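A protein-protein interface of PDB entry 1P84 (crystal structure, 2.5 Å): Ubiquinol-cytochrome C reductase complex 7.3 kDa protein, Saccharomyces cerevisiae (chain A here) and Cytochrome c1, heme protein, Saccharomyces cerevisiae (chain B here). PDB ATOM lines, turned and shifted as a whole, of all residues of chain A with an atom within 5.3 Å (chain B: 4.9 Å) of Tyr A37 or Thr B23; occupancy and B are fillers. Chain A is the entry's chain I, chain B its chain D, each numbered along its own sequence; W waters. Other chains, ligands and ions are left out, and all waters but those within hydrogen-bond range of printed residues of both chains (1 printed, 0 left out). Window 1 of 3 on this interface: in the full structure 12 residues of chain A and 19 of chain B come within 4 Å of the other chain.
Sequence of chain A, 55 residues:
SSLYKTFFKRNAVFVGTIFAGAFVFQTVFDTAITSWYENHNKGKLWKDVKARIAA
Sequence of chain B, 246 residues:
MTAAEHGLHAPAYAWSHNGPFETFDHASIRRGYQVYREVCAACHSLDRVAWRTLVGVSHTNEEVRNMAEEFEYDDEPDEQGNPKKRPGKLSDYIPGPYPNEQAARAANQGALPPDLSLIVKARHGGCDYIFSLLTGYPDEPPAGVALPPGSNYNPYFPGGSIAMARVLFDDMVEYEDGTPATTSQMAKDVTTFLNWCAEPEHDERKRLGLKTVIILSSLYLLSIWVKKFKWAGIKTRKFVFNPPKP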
ATOM      1  N   ALA A  32      22.721  26.494  -7.815  1.00  0.00           N
ATOM      2  CA  ALA A  32      22.606  25.155  -8.388  1.00  0.00           C
ATOM      3  C   ALA A  32      21.250  24.521  -8.068  1.00  0.00           C
ATOM      4  O   ALA A  32      20.624  23.927  -8.943  1.00  0.00           O
ATOM      5  CB  ALA A  32      23.738  24.260  -7.886  1.00  0.00           C
ATOM      6  N   ILE A  33      20.788  24.692  -6.827  1.00  0.00           N
ATOM      7  CA  ILE A  33      19.517  24.131  -6.381  1.00  0.00           C
ATOM      8  C   ILE A  33      18.314  24.853  -6.973  1.00  0.00           C
ATOM      9  O   ILE A  33      17.409  24.207  -7.511  1.00  0.00           O
ATOM     10  CB  ILE A  33      19.408  24.110  -4.836  1.00  0.00           C
ATOM     11  CG1 ILE A  33      20.508  23.221  -4.242  1.00  0.00           C
ATOM     12  CG2 ILE A  33      18.027  23.617  -4.398  1.00  0.00           C
ATOM     13  CD1 ILE A  33      20.473  21.790  -4.715  1.00  0.00           C
ATOM     14  N   THR A  34      18.292  26.179  -6.873  1.00  0.00           N
ATOM     15  CA  THR A  34      17.181  26.944  -7.427  1.00  0.00           C
ATOM     16  C   THR A  34      17.019  26.647  -8.924  1.00  0.00           C
ATOM     17  O   THR A  34      15.898  26.562  -9.433  1.00  0.00           O
ATOM     18  CB  THR A  34      17.384  28.449  -7.227  1.00  0.00           C
ATOM     19  OG1 THR A  34      17.474  28.738  -5.825  1.00  0.00           O
ATOM     20  CG2 THR A  34      16.224  29.236  -7.850  1.00  0.00           C
ATOM     21  N   SER A  35      18.147  26.463  -9.612  1.00  0.00           N
ATOM     22  CA  SER A  35      18.150  26.156 -11.040  1.00  0.00           C
ATOM     23  C   SER A  35      17.482  24.821 -11.307  1.00  0.00           C
ATOM     24  O   SER A  35      16.454  24.759 -11.978  1.00  0.00           O
ATOM     25  CB  SER A  35      19.579  26.114 -11.594  1.00  0.00           C
ATOM     26  OG  SER A  35      20.091  27.420 -11.778  1.00  0.00           O
ATOM     27  N   TRP A  36      18.081  23.756 -10.782  1.00  0.00           N
ATOM     28  CA  TRP A  36      17.555  22.408 -10.951  1.00  0.00           C
ATOM     29  C   TRP A  36      16.075  22.332 -10.598  1.00  0.00           C
ATOM     30  O   TRP A  36      15.291  21.715 -11.318  1.00  0.00           O
ATOM     31  CB  TRP A  36      18.337  21.427 -10.082  1.00  0.00           C
ATOM     32  CG  TRP A  36      17.855  20.024 -10.212  1.00  0.00           C
ATOM     33  CD1 TRP A  36      18.349  19.067 -11.040  1.00  0.00           C
ATOM     34  CD2 TRP A  36      16.737  19.436  -9.537  1.00  0.00           C
ATOM     35  NE1 TRP A  36      17.603  17.923 -10.940  1.00  0.00           N
ATOM     36  CE2 TRP A  36      16.606  18.121 -10.023  1.00  0.00           C
ATOM     37  CE3 TRP A  36      15.829  19.897  -8.574  1.00  0.00           C
ATOM     38  CZ2 TRP A  36      15.603  17.254  -9.577  1.00  0.00           C
ATOM     39  CZ3 TRP A  36      14.830  19.041  -8.131  1.00  0.00           C
ATOM     40  CH2 TRP A  36      14.725  17.733  -8.634  1.00  0.00           C
ATOM     41  N   TYR A  37      15.708  22.975  -9.493  1.00  0.00           N
ATOM     42  CA  TYR A  37      14.337  22.994  -8.996  1.00  0.00           C
ATOM     43  C   TYR A  37      13.363  23.625  -9.990  1.00  0.00           C
ATOM     44  O   TYR A  37      12.338  23.025 -10.318  1.00  0.00           O
ATOM     45  CB  TYR A  37      14.292  23.730  -7.644  1.00  0.00           C
ATOM     46  CG  TYR A  37      12.997  23.597  -6.867  1.00  0.00           C
ATOM     47  CD1 TYR A  37      12.617  22.375  -6.309  1.00  0.00           C
ATOM     48  CD2 TYR A  37      12.169  24.701  -6.667  1.00  0.00           C
ATOM     49  CE1 TYR A  37      11.440  22.254  -5.571  1.00  0.00           C
ATOM     50  CE2 TYR A  37      10.995  24.596  -5.934  1.00  0.00           C
ATOM     51  CZ  TYR A  37      10.636  23.371  -5.388  1.00  0.00           C
ATOM     52  OH  TYR A  37       9.483  23.265  -4.654  1.00  0.00           O
ATOM     53  N   GLU A  38      13.678  24.830 -10.463  1.00  0.00           N
ATOM     54  CA  GLU A  38      12.815  25.529 -11.424  1.00  0.00           C
ATOM     55  C   GLU A  38      12.702  24.799 -12.764  1.00  0.00           C
ATOM     56  O   GLU A  38      11.650  24.816 -13.402  1.00  0.00           O
ATOM     57  CB  GLU A  38      13.293  26.966 -11.653  1.00  0.00           C
ATOM     58  CG  GLU A  38      12.952  27.918 -10.523  1.00  0.00           C
ATOM     59  CD  GLU A  38      13.308  29.364 -10.832  1.00  0.00           C
ATOM     60  OE1 GLU A  38      12.837  30.257 -10.089  1.00  0.00           O
ATOM     61  OE2 GLU A  38      14.056  29.617 -11.807  1.00  0.00           O
ATOM     62  N   ASN A  39      13.784  24.154 -13.181  1.00  0.00           N
ATOM     63  CA  ASN A  39      13.786  23.421 -14.435  1.00  0.00           C
ATOM     64  C   ASN A  39      12.896  22.183 -14.317  1.00  0.00           C
ATOM     65  O   ASN A  39      12.173  21.838 -15.253  1.00  0.00           O
ATOM     66  CB  ASN A  39      15.214  23.015 -14.822  1.00  0.00           C
ATOM     67  CG  ASN A  39      15.274  22.324 -16.177  1.00  0.00           C
ATOM     68  OD1 ASN A  39      15.228  22.976 -17.225  1.00  0.00           O
ATOM     69  ND2 ASN A  39      15.348  20.995 -16.162  1.00  0.00           N
ATOM     70  N   HIS A  40      12.950  21.529 -13.161  1.00  0.00           N
ATOM     71  CA  HIS A  40      12.149  20.333 -12.910  1.00  0.00           C
ATOM     72  C   HIS A  40      10.658  20.660 -12.954  1.00  0.00           C
ATOM     73  O   HIS A  40       9.853  19.840 -13.381  1.00  0.00           O
ATOM     74  CB  HIS A  40      12.519  19.720 -11.546  1.00  0.00           C
ATOM     75  CG  HIS A  40      11.797  18.444 -11.237  1.00  0.00           C
ATOM     76  ND1 HIS A  40      12.274  17.207 -11.616  1.00  0.00           N
ATOM     77  CD2 HIS A  40      10.625  18.214 -10.597  1.00  0.00           C
ATOM     78  CE1 HIS A  40      11.429  16.271 -11.225  1.00  0.00           C
ATOM     79  NE2 HIS A  40      10.419  16.855 -10.606  1.00  0.00           N
ATOM     80  N   ASN A  41      10.300  21.863 -12.514  1.00  0.00           N
ATOM     81  CA  ASN A  41       8.905  22.286 -12.502  1.00  0.00           C
ATOM     82  C   ASN A  41       8.530  23.241 -13.631  1.00  0.00           C
ATOM     83  O   ASN A  41       7.573  24.001 -13.514  1.00  0.00           O
ATOM     84  CB  ASN A  41       8.543  22.901 -11.146  1.00  0.00           C
ATOM     85  CG  ASN A  41       8.422  21.858 -10.046  1.00  0.00           C
ATOM     86  OD1 ASN A  41       7.333  21.334  -9.788  1.00  0.00           O
ATOM     87  ND2 ASN A  41       9.543  21.552  -9.389  1.00  0.00           N
ATOM     88  N   LYS A  44       4.869  24.776 -14.715  1.00  0.00           N
ATOM     89  CA  LYS A  44       3.985  24.916 -13.559  1.00  0.00           C
ATOM     90  C   LYS A  44       4.115  26.239 -12.821  1.00  0.00           C
ATOM     91  O   LYS A  44       3.158  26.696 -12.184  1.00  0.00           O
ATOM     92  CB  LYS A  44       4.206  23.752 -12.590  1.00  0.00           C
ATOM     93  CG  LYS A  44       3.654  22.423 -13.086  1.00  0.00           C
ATOM     94  CD  LYS A  44       4.400  21.219 -12.502  1.00  0.00           C
ATOM     95  CE  LYS A  44       4.252  21.117 -10.995  1.00  0.00           C
ATOM     96  NZ  LYS A  44       5.042  19.979 -10.452  1.00  0.00           N
ATOM     97  N   LEU A  45       5.292  26.855 -12.924  1.00  0.00           N
ATOM     98  CA  LEU A  45       5.589  28.135 -12.265  1.00  0.00           C
ATOM     99  C   LEU A  45       4.822  29.340 -12.797  1.00  0.00           C
ATOM    100  O   LEU A  45       4.261  29.307 -13.889  1.00  0.00           O
ATOM    101  CB  LEU A  45       7.084  28.439 -12.365  1.00  0.00           C
ATOM    102  CG  LEU A  45       8.087  27.793 -11.410  1.00  0.00           C
ATOM    103  CD1 LEU A  45       7.529  26.537 -10.762  1.00  0.00           C
ATOM    104  CD2 LEU A  45       9.372  27.493 -12.169  1.00  0.00           C
ATOM    105  N   SER B  16      -0.439  16.994  -9.217  1.00  0.00           N
ATOM    106  CA  SER B  16       0.855  17.410  -9.734  1.00  0.00           C
ATOM    107  C   SER B  16       1.779  17.944  -8.634  1.00  0.00           C
ATOM    108  O   SER B  16       2.999  17.991  -8.815  1.00  0.00           O
ATOM    109  CB  SER B  16       0.687  18.417 -10.885  1.00  0.00           C
ATOM    110  OG  SER B  16      -0.214  19.458 -10.546  1.00  0.00           O
ATOM    111  N   HIS B  17       1.206  18.340  -7.497  1.00  0.00           N
ATOM    112  CA  HIS B  17       2.024  18.828  -6.387  1.00  0.00           C
ATOM    113  C   HIS B  17       2.490  17.755  -5.376  1.00  0.00           C
ATOM    114  O   HIS B  17       3.215  18.066  -4.429  1.00  0.00           O
ATOM    115  CB  HIS B  17       1.372  20.024  -5.688  1.00  0.00           C
ATOM    116  CG  HIS B  17      -0.080  19.846  -5.378  1.00  0.00           C
ATOM    117  ND1 HIS B  17      -0.536  19.513  -4.121  1.00  0.00           N
ATOM    118  CD2 HIS B  17      -1.183  20.023  -6.141  1.00  0.00           C
ATOM    119  CE1 HIS B  17      -1.857  19.494  -4.122  1.00  0.00           C
ATOM    120  NE2 HIS B  17      -2.274  19.801  -5.335  1.00  0.00           N
ATOM    121  N   PHE B  21       9.861  16.865  -4.873  1.00  0.00           N
ATOM    122  CA  PHE B  21      10.366  17.863  -5.812  1.00  0.00           C
ATOM    123  C   PHE B  21       9.317  18.614  -6.622  1.00  0.00           C
ATOM    124  O   PHE B  21       9.667  19.261  -7.605  1.00  0.00           O
ATOM    125  CB  PHE B  21      11.332  17.209  -6.804  1.00  0.00           C
ATOM    126  CG  PHE B  21      12.298  16.246  -6.179  1.00  0.00           C
ATOM    127  CD1 PHE B  21      12.402  14.946  -6.655  1.00  0.00           C
ATOM    128  CD2 PHE B  21      13.120  16.641  -5.133  1.00  0.00           C
ATOM    129  CE1 PHE B  21      13.314  14.051  -6.100  1.00  0.00           C
ATOM    130  CE2 PHE B  21      14.037  15.746  -4.572  1.00  0.00           C
ATOM    131  CZ  PHE B  21      14.133  14.452  -5.058  1.00  0.00           C
ATOM    132  N   GLU B  22       8.054  18.576  -6.208  1.00  0.00           N
ATOM    133  CA  GLU B  22       7.000  19.236  -6.987  1.00  0.00           C
ATOM    134  C   GLU B  22       6.341  20.499  -6.436  1.00  0.00           C
ATOM    135  O   GLU B  22       5.915  20.551  -5.280  1.00  0.00           O
ATOM    136  CB  GLU B  22       5.900  18.228  -7.335  1.00  0.00           C
ATOM    137  CG  GLU B  22       6.400  16.890  -7.870  1.00  0.00           C
ATOM    138  CD  GLU B  22       7.200  17.011  -9.149  1.00  0.00           C
ATOM    139  OE1 GLU B  22       8.173  16.246  -9.296  1.00  0.00           O
ATOM    140  OE2 GLU B  22       6.859  17.857 -10.009  1.00  0.00           O
ATOM    141  N   THR B  23       6.205  21.496  -7.303  1.00  0.00           N
ATOM    142  CA  THR B  23       5.563  22.758  -6.945  1.00  0.00           C
ATOM    143  C   THR B  23       4.079  22.679  -7.297  1.00  0.00           C
ATOM    144  O   THR B  23       3.647  21.746  -7.963  1.00  0.00           O
ATOM    145  CB  THR B  23       6.136  23.930  -7.762  1.00  0.00           C
ATOM    146  OG1 THR B  23       5.989  23.655  -9.162  1.00  0.00           O
ATOM    147  CG2 THR B  23       7.601  24.149  -7.444  1.00  0.00           C
ATOM    148  N   PHE B  24       3.294  23.642  -6.835  1.00  0.00           N
ATOM    149  CA  PHE B  24       1.886  23.678  -7.196  1.00  0.00           C
ATOM    150  C   PHE B  24       1.889  24.002  -8.693  1.00  0.00           C
ATOM    151  O   PHE B  24       2.929  24.354  -9.260  1.00  0.00           O
ATOM    152  CB  PHE B  24       1.169  24.842  -6.499  1.00  0.00           C
ATOM    153  CG  PHE B  24       0.738  24.563  -5.089  1.00  0.00           C
ATOM    154  CD1 PHE B  24       0.825  25.561  -4.121  1.00  0.00           C
ATOM    155  CD2 PHE B  24       0.199  23.333  -4.732  1.00  0.00           C
ATOM    156  CE1 PHE B  24       0.376  25.340  -2.820  1.00  0.00           C
ATOM    157  CE2 PHE B  24      -0.253  23.103  -3.433  1.00  0.00           C
ATOM    158  CZ  PHE B  24      -0.163  24.109  -2.477  1.00  0.00           C
ATOM    159  N   ASP B  25       0.735  23.863  -9.335  1.00  0.00           N
ATOM    160  CA  ASP B  25       0.596  24.220 -10.739  1.00  0.00           C
ATOM    161  C   ASP B  25      -0.114  25.567 -10.625  1.00  0.00           C
ATOM    162  O   ASP B  25      -1.279  25.628 -10.231  1.00  0.00           O
ATOM    163  CB  ASP B  25      -0.280  23.206 -11.462  1.00  0.00           C
ATOM    164  CG  ASP B  25      -0.399  23.487 -12.945  1.00  0.00           C
ATOM    165  OD1 ASP B  25      -0.036  22.596 -13.742  1.00  0.00           O
ATOM    166  OD2 ASP B  25      -0.867  24.584 -13.317  1.00  0.00           O
ATOM    167  N   HIS B 202       4.203  26.410   0.531  1.00  0.00           N
ATOM    168  CA  HIS B 202       4.466  25.155  -0.172  1.00  0.00           C
ATOM    169  C   HIS B 202       5.698  25.073  -1.093  1.00  0.00           C
ATOM    170  O   HIS B 202       6.652  24.361  -0.772  1.00  0.00           O
ATOM    171  CB  HIS B 202       3.201  24.717  -0.916  1.00  0.00           C
ATOM    172  CG  HIS B 202       3.329  23.406  -1.628  1.00  0.00           C
ATOM    173  ND1 HIS B 202       3.707  23.312  -2.949  1.00  0.00           N
ATOM    174  CD2 HIS B 202       3.132  22.137  -1.204  1.00  0.00           C
ATOM    175  CE1 HIS B 202       3.743  22.040  -3.307  1.00  0.00           C
ATOM    176  NE2 HIS B 202       3.397  21.306  -2.267  1.00  0.00           N
ATOM    177  N   ASP B 203       5.685  25.792  -2.218  1.00  0.00           N
ATOM    178  CA  ASP B 203       6.801  25.753  -3.186  1.00  0.00           C
ATOM    179  C   ASP B 203       8.162  26.089  -2.586  1.00  0.00           C
ATOM    180  O   ASP B 203       9.163  25.404  -2.848  1.00  0.00           O
ATOM    181  CB  ASP B 203       6.543  26.697  -4.367  1.00  0.00           C
ATOM    182  CG  ASP B 203       5.272  26.361  -5.127  1.00  0.00           C
ATOM    183  OD1 ASP B 203       4.854  25.183  -5.140  1.00  0.00           O
ATOM    184  OD2 ASP B 203       4.689  27.294  -5.712  1.00  0.00           O
ATOM    185  N   LYS B 206       9.524  23.396   0.020  1.00  0.00           N
ATOM    186  CA  LYS B 206      10.138  22.230  -0.592  1.00  0.00           C
ATOM    187  C   LYS B 206      11.512  22.504  -1.185  1.00  0.00           C
ATOM    188  O   LYS B 206      12.336  21.600  -1.283  1.00  0.00           O
ATOM    189  CB  LYS B 206       9.228  21.632  -1.647  1.00  0.00           C
ATOM    190  CG  LYS B 206       7.971  20.987  -1.100  1.00  0.00           C
ATOM    191  CD  LYS B 206       7.427  19.973  -2.085  1.00  0.00           C
ATOM    192  CE  LYS B 206       5.990  19.639  -1.770  1.00  0.00           C
ATOM    193  NZ  LYS B 206       5.474  18.592  -2.699  1.00  0.00           N
ATOM    194  N   ARG B 207      11.757  23.742  -1.602  1.00  0.00           N
ATOM    195  CA  ARG B 207      13.060  24.117  -2.159  1.00  0.00           C
ATOM    196  C   ARG B 207      14.078  24.131  -1.007  1.00  0.00           C
ATOM    197  O   ARG B 207      15.168  23.550  -1.112  1.00  0.00           O
ATOM    198  CB  ARG B 207      12.990  25.502  -2.809  1.00  0.00           C
ATOM    199  CG  ARG B 207      14.135  25.795  -3.767  1.00  0.00           C
ATOM    200  CD  ARG B 207      14.189  27.269  -4.127  1.00  0.00           C
ATOM    201  NE  ARG B 207      15.291  27.913  -3.428  1.00  0.00           N
ATOM    202  CZ  ARG B 207      15.150  28.854  -2.504  1.00  0.00           C
ATOM    203  NH1 ARG B 207      16.214  29.374  -1.906  1.00  0.00           N
ATOM    204  NH2 ARG B 207      13.946  29.293  -2.196  1.00  0.00           N
ATOM    205  N   LEU B 210      15.099  20.638   0.112  1.00  0.00           N
ATOM    206  CA  LEU B 210      16.091  19.964  -0.720  1.00  0.00           C
ATOM    207  C   LEU B 210      17.520  20.361  -0.324  1.00  0.00           C
ATOM    208  O   LEU B 210      18.415  19.519  -0.295  1.00  0.00           O
ATOM    209  CB  LEU B 210      15.819  20.272  -2.200  1.00  0.00           C
ATOM    210  CG  LEU B 210      16.739  19.638  -3.255  1.00  0.00           C
ATOM    211  CD1 LEU B 210      16.781  18.116  -3.105  1.00  0.00           C
ATOM    212  CD2 LEU B 210      16.271  20.040  -4.641  1.00  0.00           C
HETATM  213  O   HOH W   1      17.589  27.217  -3.242  1.00  0.00           O
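O of Ser B16 is in hydrogen-bond range of NZ of Lys A44, at 3.3 Å. ND2 of Asn A41 lies within hydrogen-bond range of O of Phe B21 (2.9 Å). A ring nitrogen (NE2) of His A40 is in hydrogen-bond range of the side-chain carboxylate of Glu B22, at 2.7 Å. NZ of Lys A44 is in salt-bridge range of OE2 of Glu B22 (2.8 Å). N of Thr B23 is in hydrogen-bond range of OD1 of Asn A41. The backbone carbonyl oxygen of Thr B23 sits close to the side-chain amino group of Lys A44 (3.4 Å). The backbone carbonyl oxygen of Asp B203 is in hydrogen-bond range of the side-chain hydroxyl of Tyr A37, 2.8 Å away. The guanidinium group of Arg B207 sits at hydrogen-bond distance from the side-chain hydroxyl of Thr A34 (3.3 Å).
NZ of Lys B206 lies within hydrogen-bond range of O of Glu B22, 3.3 Å away. N of Phe B24 lies within hydrogen-bond range of OD1 of Asp B203 (2.8 Å). The side-chain carboxylate (OD1) of Asp B203 is in hydrogen-bond range of a ring nitrogen (ND1) of His B202 (3.1 Å). NE2 of His B202 sits close to NZ of Lys B206. The side-chain amide nitrogen (ND2) of Asn A41 sits at hydrogen-bond distance from the backbone carbonyl oxygen (O) of Tyr A37 (3.3 Å). OD1 of Asn A41 is in hydrogen-bond range of NZ of Lys A44 (2.7 Å).
Among the printed residues, pairs that only touch across the chains: His A40 with Phe B21, Tyr A37 with Lys B206, Tyr A37 with Thr B23, Asn A41 with Glu B22, Lys A44 with Phe B24, Leu A45 with Thr B23, Tyr A37 with Arg B207, Lys A44 with Asp B25, Trp A36 with Phe B21, Trp A36 with Leu B210 and Ile A33 with Leu B210.
Tyr A37 touches just these residues of chain B: Thr B23, Asp B203, Lys B206 and Arg B207. Of the printed residues of chain A, Ser B16 touches Lys A44. Printed residues of chain A within 4 Å of Leu B210: Ile A33 (3.99 Å) and Trp A36 (3.9 Å). Printed residues of chain A within 4 Å of Asp B25: Lys A44 (3.8 Å). Printed residues of chain B within 4 Å of Thr A34: Arg B207 (3.3 Å). His B202 touches none of the printed residues of chain A. The nearest printed residue of chain B that does not touch Leu A45 is Phe B24 (5.0 Å).
Printed residues of chain A that touch a printed residue of chain B: Ile A33, Thr A34, Trp A36, Tyr A37, His A40, Asn A41, Lys A44 and Leu A45. Hydrophobic or aromatic side chains of chain B that line the printed part of chain A: Phe B21 and Leu B210. Among the printed residues, 19 pairs touch across the chains. Among the printed residues, Asp or Glu carboxylates within 4 Å of a Lys or Arg side-chain nitrogen of the other chain: Lys A44 with Glu B22.
Water W1 lies within hydrogen-bond range of NE of Arg B207 (2.4 Å) and OG1 of Thr A34 (3.0 Å).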
